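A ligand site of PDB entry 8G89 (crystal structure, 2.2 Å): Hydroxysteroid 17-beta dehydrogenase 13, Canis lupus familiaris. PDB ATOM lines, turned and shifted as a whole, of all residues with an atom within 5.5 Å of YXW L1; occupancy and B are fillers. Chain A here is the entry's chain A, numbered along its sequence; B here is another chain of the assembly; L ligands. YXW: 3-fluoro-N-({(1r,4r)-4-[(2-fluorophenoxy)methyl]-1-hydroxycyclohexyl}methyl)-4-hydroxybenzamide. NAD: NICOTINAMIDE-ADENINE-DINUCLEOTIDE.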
ATOM      1  N   PRO A 127     -16.584 -10.410  24.632  1.00  0.00           N
ATOM      2  CA  PRO A 127     -17.969 -10.069  24.272  1.00  0.00           C
ATOM      3  C   PRO A 127     -18.646 -11.165  23.445  1.00  0.00           C
ATOM      4  O   PRO A 127     -18.059 -11.671  22.480  1.00  0.00           O
ATOM      5  CB  PRO A 127     -17.804  -8.796  23.442  1.00  0.00           C
ATOM      6  CG  PRO A 127     -16.502  -8.230  23.852  1.00  0.00           C
ATOM      7  CD  PRO A 127     -15.635  -9.409  24.114  1.00  0.00           C
ATOM      8  N   ALA A 172     -12.621  -0.920  38.100  1.00  0.00           N
ATOM      9  CA  ALA A 172     -13.798  -1.691  37.771  1.00  0.00           C
ATOM     10  C   ALA A 172     -14.369  -1.204  36.381  1.00  0.00           C
ATOM     11  O   ALA A 172     -13.660  -1.397  35.389  1.00  0.00           O
ATOM     12  CB  ALA A 172     -14.797  -1.708  38.952  1.00  0.00           C
ATOM     13  N   SER A 173     -15.519  -0.500  36.281  1.00  0.00           N
ATOM     14  CA  SER A 173     -16.129  -0.037  35.056  1.00  0.00           C
ATOM     15  C   SER A 173     -17.522   0.468  35.433  1.00  0.00           C
ATOM     16  O   SER A 173     -18.001   0.145  36.526  1.00  0.00           O
ATOM     17  CB  SER A 173     -16.295  -1.231  34.099  1.00  0.00           C
ATOM     18  OG  SER A 173     -17.049  -0.920  32.930  1.00  0.00           O
ATOM     19  N   VAL A 174     -18.195   1.200  34.519  1.00  0.00           N
ATOM     20  CA  VAL A 174     -19.608   1.518  34.749  1.00  0.00           C
ATOM     21  C   VAL A 174     -20.437   0.206  34.728  1.00  0.00           C
ATOM     22  O   VAL A 174     -21.529   0.177  35.258  1.00  0.00           O
ATOM     23  CB  VAL A 174     -20.187   2.564  33.776  1.00  0.00           C
ATOM     24  CG1 VAL A 174     -19.464   3.900  33.961  1.00  0.00           C
ATOM     25  CG2 VAL A 174     -20.116   2.076  32.337  1.00  0.00           C
ATOM     26  N   CYS A 175     -19.869  -0.900  34.149  1.00  0.00           N
ATOM     27  CA  CYS A 175     -20.433  -2.244  34.125  1.00  0.00           C
ATOM     28  C   CYS A 175     -20.484  -2.906  35.512  1.00  0.00           C
ATOM     29  O   CYS A 175     -21.035  -4.004  35.613  1.00  0.00           O
ATOM     30  CB  CYS A 175     -19.689  -3.125  33.127  1.00  0.00           C
ATOM     31  SG  CYS A 175     -20.061  -2.750  31.400  1.00  0.00           S
ATOM     32  N   ILE A 180     -24.640  -4.078  30.425  1.00  0.00           N
ATOM     33  CA  ILE A 180     -24.722  -3.973  28.963  1.00  0.00           C
ATOM     34  C   ILE A 180     -24.934  -5.391  28.414  1.00  0.00           C
ATOM     35  O   ILE A 180     -24.266  -6.324  28.881  1.00  0.00           O
ATOM     36  CB  ILE A 180     -23.418  -3.356  28.391  1.00  0.00           C
ATOM     37  CG1 ILE A 180     -23.109  -1.996  29.057  1.00  0.00           C
ATOM     38  CG2 ILE A 180     -23.472  -3.244  26.864  1.00  0.00           C
ATOM     39  CD1 ILE A 180     -21.944  -1.244  28.566  1.00  0.00           C
ATOM     40  N   PRO A 181     -25.837  -5.599  27.432  1.00  0.00           N
ATOM     41  CA  PRO A 181     -25.993  -6.960  26.873  1.00  0.00           C
ATOM     42  C   PRO A 181     -24.733  -7.408  26.128  1.00  0.00           C
ATOM     43  O   PRO A 181     -23.900  -6.570  25.739  1.00  0.00           O
ATOM     44  CB  PRO A 181     -27.201  -6.834  25.929  1.00  0.00           C
ATOM     45  CG  PRO A 181     -27.297  -5.416  25.606  1.00  0.00           C
ATOM     46  CD  PRO A 181     -26.701  -4.627  26.746  1.00  0.00           C
ATOM     47  N   TYR A 182     -24.548  -8.736  25.984  1.00  0.00           N
ATOM     48  CA  TYR A 182     -23.363  -9.329  25.343  1.00  0.00           C
ATOM     49  C   TYR A 182     -22.119  -9.287  26.251  1.00  0.00           C
ATOM     50  O   TYR A 182     -21.055  -9.749  25.847  1.00  0.00           O
ATOM     51  CB  TYR A 182     -23.092  -8.723  23.942  1.00  0.00           C
ATOM     52  CG  TYR A 182     -24.347  -8.707  23.097  1.00  0.00           C
ATOM     53  CD1 TYR A 182     -25.123  -9.854  22.960  1.00  0.00           C
ATOM     54  CD2 TYR A 182     -24.857  -7.523  22.601  1.00  0.00           C
ATOM     55  CE1 TYR A 182     -26.325  -9.828  22.265  1.00  0.00           C
ATOM     56  CE2 TYR A 182     -26.053  -7.493  21.888  1.00  0.00           C
ATOM     57  CZ  TYR A 182     -26.785  -8.656  21.718  1.00  0.00           C
ATOM     58  OH  TYR A 182     -27.979  -8.662  21.030  1.00  0.00           O
ATOM     59  N   LEU A 183     -22.263  -8.801  27.491  1.00  0.00           N
ATOM     60  CA  LEU A 183     -21.177  -8.704  28.455  1.00  0.00           C
ATOM     61  C   LEU A 183     -21.616  -9.240  29.826  1.00  0.00           C
ATOM     62  O   LEU A 183     -21.197  -8.699  30.838  1.00  0.00           O
ATOM     63  CB  LEU A 183     -20.752  -7.223  28.583  1.00  0.00           C
ATOM     64  CG  LEU A 183     -20.124  -6.582  27.376  1.00  0.00           C
ATOM     65  CD1 LEU A 183     -19.812  -5.120  27.667  1.00  0.00           C
ATOM     66  CD2 LEU A 183     -18.881  -7.323  26.959  1.00  0.00           C
ATOM     67  N   TYR A 186     -18.637 -10.384  32.057  1.00  0.00           N
ATOM     68  CA  TYR A 186     -17.840  -9.191  32.321  1.00  0.00           C
ATOM     69  C   TYR A 186     -18.513  -8.252  33.334  1.00  0.00           C
ATOM     70  O   TYR A 186     -17.872  -7.832  34.297  1.00  0.00           O
ATOM     71  CB  TYR A 186     -17.555  -8.468  31.005  1.00  0.00           C
ATOM     72  CG  TYR A 186     -16.773  -7.189  31.165  1.00  0.00           C
ATOM     73  CD1 TYR A 186     -15.404  -7.216  31.386  1.00  0.00           C
ATOM     74  CD2 TYR A 186     -17.395  -5.962  31.051  1.00  0.00           C
ATOM     75  CE1 TYR A 186     -14.674  -6.043  31.493  1.00  0.00           C
ATOM     76  CE2 TYR A 186     -16.687  -4.780  31.185  1.00  0.00           C
ATOM     77  CZ  TYR A 186     -15.325  -4.826  31.399  1.00  0.00           C
ATOM     78  OH  TYR A 186     -14.618  -3.658  31.529  1.00  0.00           O
ATOM     79  N   PRO A 219     -14.905   3.815  34.518  1.00  0.00           N
ATOM     80  CA  PRO A 219     -15.135   4.552  33.258  1.00  0.00           C
ATOM     81  C   PRO A 219     -16.180   3.889  32.351  1.00  0.00           C
ATOM     82  O   PRO A 219     -16.461   2.699  32.480  1.00  0.00           O
ATOM     83  CB  PRO A 219     -13.743   4.545  32.584  1.00  0.00           C
ATOM     84  CG  PRO A 219     -12.950   3.492  33.293  1.00  0.00           C
ATOM     85  CD  PRO A 219     -13.784   2.873  34.380  1.00  0.00           C
ATOM     86  N   VAL A 220     -16.733   4.676  31.414  1.00  0.00           N
ATOM     87  CA  VAL A 220     -17.600   4.174  30.345  1.00  0.00           C
ATOM     88  C   VAL A 220     -16.607   3.589  29.262  1.00  0.00           C
ATOM     89  O   VAL A 220     -15.465   3.273  29.621  1.00  0.00           O
ATOM     90  CB  VAL A 220     -18.576   5.267  29.788  1.00  0.00           C
ATOM     91  CG1 VAL A 220     -19.654   5.627  30.801  1.00  0.00           C
ATOM     92  CG2 VAL A 220     -17.829   6.506  29.310  1.00  0.00           C
ATOM     93  N   PHE A 221     -17.005   3.388  28.000  1.00  0.00           N
ATOM     94  CA  PHE A 221     -16.104   2.861  26.975  1.00  0.00           C
ATOM     95  C   PHE A 221     -14.943   3.838  26.750  1.00  0.00           C
ATOM     96  O   PHE A 221     -15.129   5.055  26.674  1.00  0.00           O
ATOM     97  CB  PHE A 221     -16.903   2.595  25.702  1.00  0.00           C
ATOM     98  CG  PHE A 221     -16.136   2.259  24.448  1.00  0.00           C
ATOM     99  CD1 PHE A 221     -15.500   3.259  23.705  1.00  0.00           C
ATOM    100  CD2 PHE A 221     -16.144   0.979  23.935  1.00  0.00           C
ATOM    101  CE1 PHE A 221     -14.831   2.963  22.524  1.00  0.00           C
ATOM    102  CE2 PHE A 221     -15.497   0.677  22.724  1.00  0.00           C
ATOM    103  CZ  PHE A 221     -14.835   1.674  22.043  1.00  0.00           C
ATOM    104  N   PHE A 226      -9.744  -2.541  23.780  1.00  0.00           N
ATOM    105  CA  PHE A 226     -10.265  -3.517  24.719  1.00  0.00           C
ATOM    106  C   PHE A 226     -11.522  -4.219  24.196  1.00  0.00           C
ATOM    107  O   PHE A 226     -11.641  -5.433  24.319  1.00  0.00           O
ATOM    108  CB  PHE A 226     -10.495  -2.865  26.076  1.00  0.00           C
ATOM    109  CG  PHE A 226     -10.766  -3.814  27.215  1.00  0.00           C
ATOM    110  CD1 PHE A 226      -9.774  -4.682  27.656  1.00  0.00           C
ATOM    111  CD2 PHE A 226     -11.983  -3.822  27.869  1.00  0.00           C
ATOM    112  CE1 PHE A 226     -10.017  -5.547  28.715  1.00  0.00           C
ATOM    113  CE2 PHE A 226     -12.212  -4.676  28.936  1.00  0.00           C
ATOM    114  CZ  PHE A 226     -11.231  -5.541  29.341  1.00  0.00           C
ATOM    115  N   THR A 227     -12.454  -3.437  23.615  1.00  0.00           N
ATOM    116  CA  THR A 227     -13.666  -3.918  22.930  1.00  0.00           C
ATOM    117  C   THR A 227     -13.811  -3.194  21.556  1.00  0.00           C
ATOM    118  O   THR A 227     -13.184  -2.142  21.329  1.00  0.00           O
ATOM    119  CB  THR A 227     -14.930  -3.711  23.791  1.00  0.00           C
ATOM    120  OG1 THR A 227     -15.048  -2.357  24.191  1.00  0.00           O
ATOM    121  CG2 THR A 227     -14.989  -4.603  24.993  1.00  0.00           C
ATOM    122  N   LYS A 228     -14.623  -3.762  20.641  1.00  0.00           N
ATOM    123  CA  LYS A 228     -14.907  -3.159  19.321  1.00  0.00           C
ATOM    124  C   LYS A 228     -15.708  -1.844  19.545  1.00  0.00           C
ATOM    125  O   LYS A 228     -16.477  -1.751  20.516  1.00  0.00           O
ATOM    126  CB  LYS A 228     -15.725  -4.127  18.432  1.00  0.00           C
ATOM    127  CG  LYS A 228     -17.153  -4.385  18.947  1.00  0.00           C
ATOM    128  CD  LYS A 228     -17.987  -5.301  18.086  1.00  0.00           C
ATOM    129  CE  LYS A 228     -19.079  -5.931  18.910  1.00  0.00           C
ATOM    130  NZ  LYS A 228     -18.507  -6.812  19.983  1.00  0.00           N
ATOM    131  N   ASN A 229     -15.490  -0.837  18.683  1.00  0.00           N
ATOM    132  CA  ASN A 229     -16.171   0.444  18.864  1.00  0.00           C
ATOM    133  C   ASN A 229     -17.687   0.295  18.769  1.00  0.00           C
ATOM    134  O   ASN A 229     -18.177  -0.472  17.951  1.00  0.00           O
ATOM    135  CB  ASN A 229     -15.645   1.474  17.885  1.00  0.00           C
ATOM    136  CG  ASN A 229     -14.556   2.338  18.475  1.00  0.00           C
ATOM    137  OD1 ASN A 229     -13.565   1.833  19.042  1.00  0.00           O
ATOM    138  ND2 ASN A 229     -14.715   3.651  18.355  1.00  0.00           N
ATOM    139  N   PRO A 230     -18.452   1.038  19.598  1.00  0.00           N
ATOM    140  CA  PRO A 230     -19.908   0.915  19.561  1.00  0.00           C
ATOM    141  C   PRO A 230     -20.573   2.135  18.880  1.00  0.00           C
ATOM    142  O   PRO A 230     -19.910   2.927  18.195  1.00  0.00           O
ATOM    143  CB  PRO A 230     -20.246   0.860  21.055  1.00  0.00           C
ATOM    144  CG  PRO A 230     -19.171   1.804  21.680  1.00  0.00           C
ATOM    145  CD  PRO A 230     -18.044   1.968  20.663  1.00  0.00           C
ATOM    146  N   THR A 232     -22.585   4.272  20.869  1.00  0.00           N
ATOM    147  CA  THR A 232     -23.024   4.982  22.083  1.00  0.00           C
ATOM    148  C   THR A 232     -23.101   6.511  21.899  1.00  0.00           C
ATOM    149  O   THR A 232     -22.071   7.190  21.908  1.00  0.00           O
ATOM    150  CB  THR A 232     -22.156   4.596  23.283  1.00  0.00           C
ATOM    151  OG1 THR A 232     -20.819   5.062  23.067  1.00  0.00           O
ATOM    152  CG2 THR A 232     -22.164   3.105  23.544  1.00  0.00           C
ATOM    153  N   TRP A 235     -23.112   8.285  26.128  1.00  0.00           N
ATOM    154  CA  TRP A 235     -21.802   8.241  26.780  1.00  0.00           C
ATOM    155  C   TRP A 235     -20.724   8.648  25.770  1.00  0.00           C
ATOM    156  O   TRP A 235     -20.816   8.310  24.591  1.00  0.00           O
ATOM    157  CB  TRP A 235     -21.467   6.815  27.269  1.00  0.00           C
ATOM    158  CG  TRP A 235     -22.394   6.208  28.274  1.00  0.00           C
ATOM    159  CD1 TRP A 235     -23.338   6.857  29.032  1.00  0.00           C
ATOM    160  CD2 TRP A 235     -22.434   4.825  28.667  1.00  0.00           C
ATOM    161  NE1 TRP A 235     -23.982   5.957  29.849  1.00  0.00           N
ATOM    162  CE2 TRP A 235     -23.440   4.705  29.649  1.00  0.00           C
ATOM    163  CE3 TRP A 235     -21.711   3.684  28.295  1.00  0.00           C
ATOM    164  CZ2 TRP A 235     -23.751   3.472  30.244  1.00  0.00           C
ATOM    165  CZ3 TRP A 235     -22.011   2.473  28.888  1.00  0.00           C
ATOM    166  CH2 TRP A 235     -23.016   2.379  29.854  1.00  0.00           C
ATOM    167  N   ASN A 287     -28.415   3.050  21.201  1.00  0.00           N
ATOM    168  CA  ASN A 287     -28.261   1.958  20.247  1.00  0.00           C
ATOM    169  C   ASN A 287     -28.259   2.489  18.813  1.00  0.00           C
ATOM    170  O   ASN A 287     -27.655   3.520  18.530  1.00  0.00           O
ATOM    171  CB  ASN A 287     -29.399   0.932  20.424  1.00  0.00           C
ATOM    172  CG  ASN A 287     -29.190  -0.387  19.717  1.00  0.00           C
ATOM    173  OD1 ASN A 287     -28.080  -0.724  19.271  1.00  0.00           O
ATOM    174  ND2 ASN A 287     -30.255  -1.174  19.596  1.00  0.00           N
ATOM    175  N   THR B 206     -33.018  -7.441  25.099  1.00  0.00           N
ATOM    176  CA  THR B 206     -32.329  -7.045  23.867  1.00  0.00           C
ATOM    177  C   THR B 206     -32.501  -8.084  22.760  1.00  0.00           C
ATOM    178  O   THR B 206     -32.687  -7.717  21.592  1.00  0.00           O
ATOM    179  CB  THR B 206     -30.866  -6.728  24.145  1.00  0.00           C
ATOM    180  OG1 THR B 206     -30.785  -5.801  25.228  1.00  0.00           O
ATOM    181  CG2 THR B 206     -30.162  -6.154  22.927  1.00  0.00           C
HETATM  182  C4  YXW L   1     -26.390  -4.040  20.988  1.00  0.00           C
HETATM  183  C6  YXW L   1     -28.329  -3.099  21.992  1.00  0.00           C
HETATM  184  C9  YXW L   1     -23.470  -4.109  23.175  1.00  0.00           C
HETATM  185  C13 YXW L   1     -20.125  -3.169  21.458  1.00  0.00           C
HETATM  186  C20 YXW L   1     -18.449  -1.090  25.639  1.00  0.00           C
HETATM  187  C18 YXW L   1     -19.125  -1.998  23.461  1.00  0.00           C
HETATM  188  C16 YXW L   1     -21.118  -4.485  23.899  1.00  0.00           C
HETATM  189  O17 YXW L   1     -17.890  -3.562  22.138  1.00  0.00           O
HETATM  190  C26 YXW L   1     -16.267  -2.370  28.508  1.00  0.00           C
HETATM  191  C1  YXW L   1     -27.590  -2.798  23.113  1.00  0.00           C
HETATM  192  C2  YXW L   1     -26.247  -3.121  23.182  1.00  0.00           C
HETATM  193  C3  YXW L   1     -25.638  -3.754  22.108  1.00  0.00           C
HETATM  194  C5  YXW L   1     -27.730  -3.728  20.906  1.00  0.00           C
HETATM  195  F7  YXW L   1     -25.781  -4.634  19.934  1.00  0.00           F
HETATM  196  O8  YXW L   1     -24.338  -4.206  22.036  1.00  0.00           O
HETATM  197  C10 YXW L   1     -22.043  -4.323  22.703  1.00  0.00           C
HETATM  198  C12 YXW L   1     -21.608  -3.144  21.824  1.00  0.00           C
HETATM  199  C14 YXW L   1     -19.206  -3.322  22.675  1.00  0.00           C
HETATM  200  C15 YXW L   1     -19.654  -4.552  23.473  1.00  0.00           C
HETATM  201  N19 YXW L   1     -18.386  -2.062  24.724  1.00  0.00           N
HETATM  202  O21 YXW L   1     -19.034  -0.030  25.424  1.00  0.00           O
HETATM  203  C22 YXW L   1     -17.809  -1.332  26.968  1.00  0.00           C
HETATM  204  C23 YXW L   1     -18.275  -0.523  28.001  1.00  0.00           C
HETATM  205  C24 YXW L   1     -17.721  -0.658  29.249  1.00  0.00           C
HETATM  206  C25 YXW L   1     -16.727  -1.568  29.541  1.00  0.00           C
HETATM  207  C27 YXW L   1     -16.793  -2.252  27.232  1.00  0.00           C
HETATM  208  O28 YXW L   1     -16.220  -1.702  30.796  1.00  0.00           O
HETATM  209  F29 YXW L   1     -18.124   0.174  30.233  1.00  0.00           F
HETATM  210  PA  NAD L   2      -6.025  -2.717  27.208  1.00  0.00           P
HETATM  211  O1A NAD L   2      -5.666  -1.393  26.672  1.00  0.00           O
HETATM  212  O2A NAD L   2      -6.356  -3.847  26.307  1.00  0.00           O
HETATM  213  O5B NAD L   2      -4.869  -3.189  28.206  1.00  0.00           O
HETATM  214  C5B NAD L   2      -5.135  -4.190  29.205  1.00  0.00           C
HETATM  215  C4B NAD L   2      -3.806  -4.739  29.649  1.00  0.00           C
HETATM  216  O4B NAD L   2      -4.005  -5.777  30.630  1.00  0.00           O
HETATM  217  C3B NAD L   2      -2.975  -5.365  28.513  1.00  0.00           C
HETATM  218  O3B NAD L   2      -1.642  -4.842  28.481  1.00  0.00           O
HETATM  219  C2B NAD L   2      -3.035  -6.856  28.821  1.00  0.00           C
HETATM  220  O2B NAD L   2      -1.887  -7.611  28.368  1.00  0.00           O
HETATM  221  C1B NAD L   2      -3.093  -6.814  30.346  1.00  0.00           C
HETATM  222  N9A NAD L   2      -3.571  -8.052  30.948  1.00  0.00           N
HETATM  223  C8A NAD L   2      -4.600  -8.838  30.493  1.00  0.00           C
HETATM  224  N7A NAD L   2      -4.712  -9.987  31.110  1.00  0.00           N
HETATM  225  C5A NAD L   2      -3.675  -9.956  32.032  1.00  0.00           C
HETATM  226  C6A NAD L   2      -3.215 -10.907  32.975  1.00  0.00           C
HETATM  227  N6A NAD L   2      -3.726 -12.139  33.102  1.00  0.00           N
HETATM  228  N1A NAD L   2      -2.149 -10.565  33.729  1.00  0.00           N
HETATM  229  C2A NAD L   2      -1.581  -9.367  33.549  1.00  0.00           C
HETATM  230  N3A NAD L   2      -1.924  -8.410  32.690  1.00  0.00           N
HETATM  231  C4A NAD L   2      -2.974  -8.763  31.949  1.00  0.00           C
HETATM  232  O3  NAD L   2      -7.261  -2.508  28.198  1.00  0.00           O
HETATM  233  PN  NAD L   2      -7.821  -1.223  28.962  1.00  0.00           P
HETATM  234  O1N NAD L   2      -6.704  -0.380  29.427  1.00  0.00           O
HETATM  235  O2N NAD L   2      -8.903  -0.634  28.145  1.00  0.00           O
HETATM  236  O5D NAD L   2      -8.448  -1.911  30.266  1.00  0.00           O
HETATM  237  C5D NAD L   2      -7.822  -1.807  31.562  1.00  0.00           C
HETATM  238  C4D NAD L   2      -8.862  -2.003  32.622  1.00  0.00           C
HETATM  239  O4D NAD L   2      -9.906  -1.011  32.484  1.00  0.00           O
HETATM  240  C3D NAD L   2      -9.559  -3.362  32.636  1.00  0.00           C
HETATM  241  O3D NAD L   2      -9.758  -3.784  33.984  1.00  0.00           O
HETATM  242  C2D NAD L   2     -10.895  -3.059  31.949  1.00  0.00           C
HETATM  243  O2D NAD L   2     -11.909  -3.992  32.276  1.00  0.00           O
HETATM  244  C1D NAD L   2     -11.162  -1.652  32.472  1.00  0.00           C
HETATM  245  N1N NAD L   2     -12.075  -0.864  31.662  1.00  0.00           N
HETATM  246  C2N NAD L   2     -11.865  -0.689  30.303  1.00  0.00           C
HETATM  247  C3N NAD L   2     -12.734  -0.019  29.513  1.00  0.00           C
HETATM  248  C7N NAD L   2     -12.476   0.217  28.077  1.00  0.00           C
HETATM  249  O7N NAD L   2     -13.397   0.566  27.325  1.00  0.00           O
HETATM  250  N7N NAD L   2     -11.267  -0.068  27.601  1.00  0.00           N
HETATM  251  C4N NAD L   2     -14.058   0.434  30.053  1.00  0.00           C
HETATM  252  C5N NAD L   2     -14.033   0.463  31.549  1.00  0.00           C
HETATM  253  C6N NAD L   2     -13.176  -0.284  32.242  1.00  0.00           C
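The side-chain sulfur (SG) of Cys 175 sits close to a fluorine (F29) of YXW L1, 3.7 Å away.
Val 174 touches YXW L1 (CG2 to F29, 3.5 Å).
Ile 180 touches YXW L1.
Pro 181 touches YXW L1.
CD2 of Tyr 182 touches O8 of YXW L1, at 3.4 Å.
Pro 219 touches YXW L1.
Val 220 touches YXW L1 (C to F29, 3.9 Å).
CB of Phe 221 touches O21 of YXW L1, at 3.4 Å.
Pro 230 touches YXW L1.
Asn 287 touches YXW L1 (OD1 to C5, 3.4 Å).
Thr 206 of chain B touches YXW L1.
Hydrophobic or aromatic side chains that line YXW L1: Val 174, Ile 180, Pro 181, Tyr 182, Tyr 186, Phe 221 and Pro 230.
Within 4 Å of YXW L1: Ser 173, Val 174, Cys 175, Ile 180, Pro 181, Tyr 182, Tyr 186, Pro 219, Val 220, Phe 221, Thr 227, Lys 228, Pro 230, Asn 287 and Thr 206 of chain B.
The nearest printed residue that does not touch YXW L1 is Leu 183 (4.04 Å).
N of Val 174 lies within hydrogen-bond range of O of Pro 219 (3.1 Å).
The backbone NH of Cys 175 sits close to the side-chain hydroxyl of Ser 173, at 3.1 Å.
O of Lys 228 is in hydrogen-bond range of O17 of YXW L1, at 2.8 Å.
An oxygen (O28) of YXW L1 is in hydrogen-bond range of the side-chain hydroxyl (OG) of Ser 173 (2.4 Å).
The side-chain hydroxyl (OH) of Tyr 186 is in hydrogen-bond range of an oxygen (O2D) of NAD L2.
The side-chain hydroxyl (OG1) of Thr 227 lies within hydrogen-bond range of a nitrogen (N19) of YXW L1 (3.4 Å).
O28 of YXW L1 is in hydrogen-bond range of OH of Tyr 186.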
